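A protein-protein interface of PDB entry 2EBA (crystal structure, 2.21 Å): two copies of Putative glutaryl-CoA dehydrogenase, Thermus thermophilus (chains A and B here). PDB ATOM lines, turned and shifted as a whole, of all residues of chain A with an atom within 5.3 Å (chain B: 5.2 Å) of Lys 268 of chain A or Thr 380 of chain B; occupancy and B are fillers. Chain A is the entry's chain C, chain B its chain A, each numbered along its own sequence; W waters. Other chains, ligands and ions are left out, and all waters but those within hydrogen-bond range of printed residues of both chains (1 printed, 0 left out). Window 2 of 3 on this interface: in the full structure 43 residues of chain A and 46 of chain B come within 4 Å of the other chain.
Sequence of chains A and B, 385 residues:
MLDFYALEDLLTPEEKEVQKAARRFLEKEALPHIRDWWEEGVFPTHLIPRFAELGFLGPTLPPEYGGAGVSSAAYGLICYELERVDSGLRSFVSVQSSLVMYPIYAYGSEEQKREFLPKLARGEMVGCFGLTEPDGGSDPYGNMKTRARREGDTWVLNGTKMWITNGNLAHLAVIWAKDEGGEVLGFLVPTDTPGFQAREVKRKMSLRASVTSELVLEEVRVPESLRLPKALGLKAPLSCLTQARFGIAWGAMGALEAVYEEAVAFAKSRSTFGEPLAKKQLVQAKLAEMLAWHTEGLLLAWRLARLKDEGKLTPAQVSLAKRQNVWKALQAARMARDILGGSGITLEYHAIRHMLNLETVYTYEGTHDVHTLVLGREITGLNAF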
ATOM      1  N   ALA A 263      19.412   8.241  -3.939  1.00  0.00           N
ATOM      2  CA  ALA A 263      18.913   8.906  -2.752  1.00  0.00           C
ATOM      3  C   ALA A 263      18.086   8.004  -1.849  1.00  0.00           C
ATOM      4  O   ALA A 263      18.216   8.110  -0.620  1.00  0.00           O
ATOM      5  CB  ALA A 263      18.123  10.137  -3.110  1.00  0.00           C
ATOM      6  N   VAL A 264      17.239   7.122  -2.383  1.00  0.00           N
ATOM      7  CA  VAL A 264      16.490   6.311  -1.429  1.00  0.00           C
ATOM      8  C   VAL A 264      17.493   5.411  -0.695  1.00  0.00           C
ATOM      9  O   VAL A 264      17.313   5.166   0.497  1.00  0.00           O
ATOM     10  CB  VAL A 264      15.309   5.507  -2.061  1.00  0.00           C
ATOM     11  CG1 VAL A 264      14.871   6.165  -3.359  1.00  0.00           C
ATOM     12  CG2 VAL A 264      15.694   4.066  -2.229  1.00  0.00           C
ATOM     13  N   ALA A 265      18.567   4.972  -1.358  1.00  0.00           N
ATOM     14  CA  ALA A 265      19.577   4.133  -0.708  1.00  0.00           C
ATOM     15  C   ALA A 265      20.251   4.885   0.454  1.00  0.00           C
ATOM     16  O   ALA A 265      20.482   4.310   1.531  1.00  0.00           O
ATOM     17  CB  ALA A 265      20.637   3.704  -1.712  1.00  0.00           C
ATOM     18  N   PHE A 266      20.594   6.151   0.208  1.00  0.00           N
ATOM     19  CA  PHE A 266      21.225   6.984   1.211  1.00  0.00           C
ATOM     20  C   PHE A 266      20.195   7.174   2.332  1.00  0.00           C
ATOM     21  O   PHE A 266      20.480   6.919   3.501  1.00  0.00           O
ATOM     22  CB  PHE A 266      21.548   8.333   0.604  1.00  0.00           C
ATOM     23  CG  PHE A 266      22.439   9.183   1.435  1.00  0.00           C
ATOM     24  CD1 PHE A 266      23.815   8.970   1.440  1.00  0.00           C
ATOM     25  CD2 PHE A 266      21.916  10.254   2.152  1.00  0.00           C
ATOM     26  CE1 PHE A 266      24.656   9.807   2.148  1.00  0.00           C
ATOM     27  CE2 PHE A 266      22.746  11.100   2.875  1.00  0.00           C
ATOM     28  CZ  PHE A 266      24.125  10.880   2.865  1.00  0.00           C
ATOM     29  N   ALA A 267      18.992   7.607   1.965  1.00  0.00           N
ATOM     30  CA  ALA A 267      17.950   7.835   2.960  1.00  0.00           C
ATOM     31  C   ALA A 267      17.728   6.599   3.866  1.00  0.00           C
ATOM     32  O   ALA A 267      17.568   6.745   5.081  1.00  0.00           O
ATOM     33  CB  ALA A 267      16.660   8.228   2.278  1.00  0.00           C
ATOM     34  N   LYS A 268      17.715   5.390   3.302  1.00  0.00           N
ATOM     35  CA  LYS A 268      17.516   4.186   4.112  1.00  0.00           C
ATOM     36  C   LYS A 268      18.768   3.862   4.936  1.00  0.00           C
ATOM     37  O   LYS A 268      18.679   3.196   5.959  1.00  0.00           O
ATOM     38  CB  LYS A 268      17.212   2.966   3.223  1.00  0.00           C
ATOM     39  CG  LYS A 268      15.886   2.975   2.436  1.00  0.00           C
ATOM     40  CD  LYS A 268      16.062   2.127   1.154  1.00  0.00           C
ATOM     41  CE  LYS A 268      14.937   1.122   0.918  1.00  0.00           C
ATOM     42  NZ  LYS A 268      14.904   0.050   1.954  1.00  0.00           N
ATOM     43  N   SER A 269      19.946   4.329   4.511  1.00  0.00           N
ATOM     44  CA  SER A 269      21.212   3.996   5.193  1.00  0.00           C
ATOM     45  C   SER A 269      21.718   4.925   6.276  1.00  0.00           C
ATOM     46  O   SER A 269      22.590   4.531   7.087  1.00  0.00           O
ATOM     47  CB  SER A 269      22.341   3.869   4.165  1.00  0.00           C
ATOM     48  OG  SER A 269      22.709   5.150   3.626  1.00  0.00           O
ATOM     49  N   ARG A 270      21.186   6.142   6.323  1.00  0.00           N
ATOM     50  CA  ARG A 270      21.714   7.158   7.206  1.00  0.00           C
ATOM     51  C   ARG A 270      20.606   7.556   8.161  1.00  0.00           C
ATOM     52  O   ARG A 270      19.432   7.234   7.880  1.00  0.00           O
ATOM     53  CB  ARG A 270      22.157   8.305   6.305  1.00  0.00           C
ATOM     54  CG  ARG A 270      23.016   9.356   6.942  1.00  0.00           C
ATOM     55  CD  ARG A 270      24.476   9.223   6.505  1.00  0.00           C
ATOM     56  NE  ARG A 270      24.899  10.399   5.747  1.00  0.00           N
ATOM     57  CZ  ARG A 270      25.113  11.611   6.275  1.00  0.00           C
ATOM     58  NH1 ARG A 270      24.951  11.825   7.584  1.00  0.00           N
ATOM     59  NH2 ARG A 270      25.451  12.628   5.489  1.00  0.00           N
ATOM     60  N   PRO A 276      15.044   6.601  10.361  1.00  0.00           N
ATOM     61  CA  PRO A 276      16.136   6.690   9.364  1.00  0.00           C
ATOM     62  C   PRO A 276      15.734   7.939   8.622  1.00  0.00           C
ATOM     63  O   PRO A 276      14.689   8.522   8.909  1.00  0.00           O
ATOM     64  CB  PRO A 276      15.971   5.435   8.525  1.00  0.00           C
ATOM     65  CG  PRO A 276      15.375   4.522   9.465  1.00  0.00           C
ATOM     66  CD  PRO A 276      14.271   5.378  10.054  1.00  0.00           C
ATOM     67  N   LEU A 277      16.542   8.351   7.666  1.00  0.00           N
ATOM     68  CA  LEU A 277      16.137   9.512   6.921  1.00  0.00           C
ATOM     69  C   LEU A 277      14.872   9.138   6.163  1.00  0.00           C
ATOM     70  O   LEU A 277      13.902   9.882   6.199  1.00  0.00           O
ATOM     71  CB  LEU A 277      17.245   9.905   5.960  1.00  0.00           C
ATOM     72  CG  LEU A 277      17.858  11.281   6.186  1.00  0.00           C
ATOM     73  CD1 LEU A 277      17.531  11.814   7.578  1.00  0.00           C
ATOM     74  CD2 LEU A 277      19.360  11.170   5.944  1.00  0.00           C
ATOM     75  N   ALA A 278      14.875   7.958   5.533  1.00  0.00           N
ATOM     76  CA  ALA A 278      13.763   7.461   4.724  1.00  0.00           C
ATOM     77  C   ALA A 278      12.409   7.446   5.388  1.00  0.00           C
ATOM     78  O   ALA A 278      11.388   7.349   4.714  1.00  0.00           O
ATOM     79  CB  ALA A 278      14.077   6.064   4.220  1.00  0.00           C
ATOM     80  N   LYS A 279      12.394   7.550   6.710  1.00  0.00           N
ATOM     81  CA  LYS A 279      11.139   7.517   7.439  1.00  0.00           C
ATOM     82  C   LYS A 279      10.548   8.877   7.787  1.00  0.00           C
ATOM     83  O   LYS A 279       9.394   8.950   8.233  1.00  0.00           O
ATOM     84  CB  LYS A 279      11.297   6.707   8.721  1.00  0.00           C
ATOM     85  CG  LYS A 279       9.970   6.332   9.348  1.00  0.00           C
ATOM     86  CD  LYS A 279      10.138   5.578  10.650  1.00  0.00           C
ATOM     87  CE  LYS A 279       8.785   5.224  11.235  1.00  0.00           C
ATOM     88  NZ  LYS A 279       8.924   4.475  12.499  1.00  0.00           N
ATOM     89  N   GLN A 284      10.504  11.520   2.734  1.00  0.00           N
ATOM     90  CA  GLN A 284       9.570  10.673   1.982  1.00  0.00           C
ATOM     91  C   GLN A 284       8.921  11.454   0.831  1.00  0.00           C
ATOM     92  O   GLN A 284       8.799  10.947  -0.282  1.00  0.00           O
ATOM     93  CB  GLN A 284       8.472  10.107   2.883  1.00  0.00           C
ATOM     94  CG  GLN A 284       8.953   8.916   3.684  1.00  0.00           C
ATOM     95  CD  GLN A 284       7.877   7.897   3.969  1.00  0.00           C
ATOM     96  OE1 GLN A 284       8.176   6.764   4.376  1.00  0.00           O
ATOM     97  NE2 GLN A 284       6.609   8.286   3.771  1.00  0.00           N
ATOM     98  N   LEU A 287      11.065  11.961  -2.355  1.00  0.00           N
ATOM     99  CA  LEU A 287      11.187  10.712  -3.086  1.00  0.00           C
ATOM    100  C   LEU A 287       9.889  10.366  -3.827  1.00  0.00           C
ATOM    101  O   LEU A 287       9.938   9.867  -4.956  1.00  0.00           O
ATOM    102  CB  LEU A 287      11.592   9.570  -2.129  1.00  0.00           C
ATOM    103  CG  LEU A 287      12.886   9.754  -1.314  1.00  0.00           C
ATOM    104  CD1 LEU A 287      13.131   8.458  -0.503  1.00  0.00           C
ATOM    105  CD2 LEU A 287      14.095   9.980  -2.253  1.00  0.00           C
ATOM    106  N   LEU B 375       2.899   6.396  -0.943  1.00  0.00           N
ATOM    107  CA  LEU B 375       4.033   6.247  -1.837  1.00  0.00           C
ATOM    108  C   LEU B 375       5.336   6.168  -1.035  1.00  0.00           C
ATOM    109  O   LEU B 375       6.176   5.299  -1.283  1.00  0.00           O
ATOM    110  CB  LEU B 375       4.075   7.426  -2.821  1.00  0.00           C
ATOM    111  CG  LEU B 375       2.901   7.541  -3.806  1.00  0.00           C
ATOM    112  CD1 LEU B 375       2.990   8.848  -4.593  1.00  0.00           C
ATOM    113  CD2 LEU B 375       2.910   6.331  -4.745  1.00  0.00           C
ATOM    114  N   GLY B 376       5.496   7.069  -0.063  1.00  0.00           N
ATOM    115  CA  GLY B 376       6.698   7.070   0.748  1.00  0.00           C
ATOM    116  C   GLY B 376       6.952   5.734   1.397  1.00  0.00           C
ATOM    117  O   GLY B 376       8.054   5.193   1.347  1.00  0.00           O
ATOM    118  N   ARG B 377       5.926   5.186   2.017  1.00  0.00           N
ATOM    119  CA  ARG B 377       6.047   3.910   2.665  1.00  0.00           C
ATOM    120  C   ARG B 377       6.383   2.839   1.628  1.00  0.00           C
ATOM    121  O   ARG B 377       7.086   1.862   1.911  1.00  0.00           O
ATOM    122  CB  ARG B 377       4.747   3.562   3.341  1.00  0.00           C
ATOM    123  CG  ARG B 377       4.849   2.275   4.066  1.00  0.00           C
ATOM    124  CD  ARG B 377       3.617   1.508   3.800  1.00  0.00           C
ATOM    125  NE  ARG B 377       2.609   1.787   4.804  1.00  0.00           N
ATOM    126  CZ  ARG B 377       1.325   1.987   4.525  1.00  0.00           C
ATOM    127  NH1 ARG B 377       0.899   1.960   3.258  1.00  0.00           N
ATOM    128  NH2 ARG B 377       0.459   2.161   5.518  1.00  0.00           N
ATOM    129  N   GLU B 378       5.851   3.014   0.432  1.00  0.00           N
ATOM    130  CA  GLU B 378       6.073   2.066  -0.631  1.00  0.00           C
ATOM    131  C   GLU B 378       7.509   2.029  -1.046  1.00  0.00           C
ATOM    132  O   GLU B 378       8.108   0.972  -1.278  1.00  0.00           O
ATOM    133  CB  GLU B 378       5.308   2.502  -1.822  1.00  0.00           C
ATOM    134  CG  GLU B 378       4.522   1.410  -2.360  1.00  0.00           C
ATOM    135  CD  GLU B 378       5.237   0.657  -3.438  1.00  0.00           C
ATOM    136  OE1 GLU B 378       4.487   0.079  -4.236  1.00  0.00           O
ATOM    137  OE2 GLU B 378       6.496   0.631  -3.513  1.00  0.00           O
ATOM    138  N   ILE B 379       8.032   3.228  -1.201  1.00  0.00           N
ATOM    139  CA  ILE B 379       9.391   3.390  -1.640  1.00  0.00           C
ATOM    140  C   ILE B 379      10.434   2.972  -0.609  1.00  0.00           C
ATOM    141  O   ILE B 379      11.406   2.285  -0.936  1.00  0.00           O
ATOM    142  CB  ILE B 379       9.595   4.853  -2.056  1.00  0.00           C
ATOM    143  CG1 ILE B 379       8.644   5.181  -3.215  1.00  0.00           C
ATOM    144  CG2 ILE B 379      11.028   5.099  -2.427  1.00  0.00           C
ATOM    145  CD1 ILE B 379       8.480   6.673  -3.484  1.00  0.00           C
ATOM    146  N   THR B 380      10.221   3.360   0.639  1.00  0.00           N
ATOM    147  CA  THR B 380      11.192   3.074   1.689  1.00  0.00           C
ATOM    148  C   THR B 380      10.922   1.849   2.530  1.00  0.00           C
ATOM    149  O   THR B 380      11.828   1.325   3.171  1.00  0.00           O
ATOM    150  CB  THR B 380      11.306   4.270   2.643  1.00  0.00           C
ATOM    151  OG1 THR B 380      10.098   4.383   3.398  1.00  0.00           O
ATOM    152  CG2 THR B 380      11.517   5.546   1.869  1.00  0.00           C
ATOM    153  N   GLY B 381       9.679   1.392   2.532  1.00  0.00           N
ATOM    154  CA  GLY B 381       9.321   0.250   3.344  1.00  0.00           C
ATOM    155  C   GLY B 381       9.100   0.711   4.776  1.00  0.00           C
ATOM    156  O   GLY B 381       8.803  -0.098   5.653  1.00  0.00           O
ATOM    157  N   LEU B 382       9.244   2.014   5.012  1.00  0.00           N
ATOM    158  CA  LEU B 382       9.065   2.575   6.348  1.00  0.00           C
ATOM    159  C   LEU B 382       7.774   3.362   6.471  1.00  0.00           C
ATOM    160  O   LEU B 382       7.425   4.141   5.591  1.00  0.00           O
ATOM    161  CB  LEU B 382      10.251   3.475   6.716  1.00  0.00           C
ATOM    162  CG  LEU B 382      11.625   2.805   6.629  1.00  0.00           C
ATOM    163  CD1 LEU B 382      12.705   3.757   7.125  1.00  0.00           C
ATOM    164  CD2 LEU B 382      11.625   1.534   7.446  1.00  0.00           C
HETATM  165  O   HOH W   1       4.897   6.495   5.165  1.00  0.00           O
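The side-chain amide oxygen (OE1) of Gln 284 of chain A sits close to the backbone carbonyl oxygen (O) of Gly 376 of chain B. OG1 of Thr 380 of chain B lies close to O of Ala 278 of chain A, 3.5 Å away. The side-chain amide oxygen (OE1) of Gln 284 of chain A lies within hydrogen-bond range of the side-chain hydroxyl (OG1) of Thr 380 of chain B (3.2 Å). The backbone carbonyl oxygen of Leu 382 of chain B lies close to the side-chain amide oxygen of Gln 284 of chain A (3.0 Å).
The backbone carbonyl oxygen of Gly 376 of chain B lies within hydrogen-bond range of the side-chain hydroxyl of Thr 380 of chain B (3.0 Å). N of Leu 382 of chain B is in hydrogen-bond range of OG1 of Thr 380 of chain B (3.0 Å). The backbone carbonyl oxygen (O) of Ala 267 of chain A sits at hydrogen-bond distance from the backbone NH (N) of Ala 278 of chain A, at 3.0 Å. The side-chain amide oxygen (OE1) of Gln 284 of chain A sits close to the backbone carbonyl oxygen (O) of Ala 278 of chain A.
Lys 268 of chain A touches Thr 380 of chain B (NZ to O, 3.5 Å). CG of Pro 276 of chain A touches CD1 of Leu 382 of chain B (3.6 Å). Leu 382 of chain B touches Ala 278 of chain A. Leu 382 of chain B touches Lys 279 of chain A. Gln 284 of chain A touches Arg 377 of chain B. O of Leu 287 of chain A touches CD1 of Ile 379 of chain B (3.8 Å).
Arg 270 of chain A touches none of the printed residues of chain B. Printed residues of chain B within 4 Å of Leu 287 of chain A: Ile 379. Of chain A, only Lys 268 (3.5 Å), Ala 278 (3.4 Å) and Gln 284 (3.2 Å) come within 4 Å of Thr 380 of chain B. Printed residues of chain A within 4 Å of Leu 382 of chain B: Pro 276 (3.6 Å), Ala 278 (3.96 Å), Lys 279 (3.6 Å) and Gln 284 (3.0 Å). The nearest residue of chain B that does not touch Lys 268 of chain A is Ile 379 of chain B (4.2 Å). The nearest residue of chain A that does not touch Thr 380 of chain B is Leu 287 of chain A (4.1 Å). The nearest printed residue of chain A that does not touch Arg 377 of chain B is Ala 278 of chain A (6.5 Å).
Of the 8 printed residues of chain B, 5 touch a printed residue of chain A.
No position is printed for both chains. Of the 10 pairs that touch across the chains among the printed residues, none has its exchanged pair printed and touching as well.
Water W1 bridges the side-chain amide nitrogen (NE2) of Gln 284 of chain A (2.8 Å) and the backbone carbonyl oxygen (O) of Leu 382 of chain B (3.5 Å).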
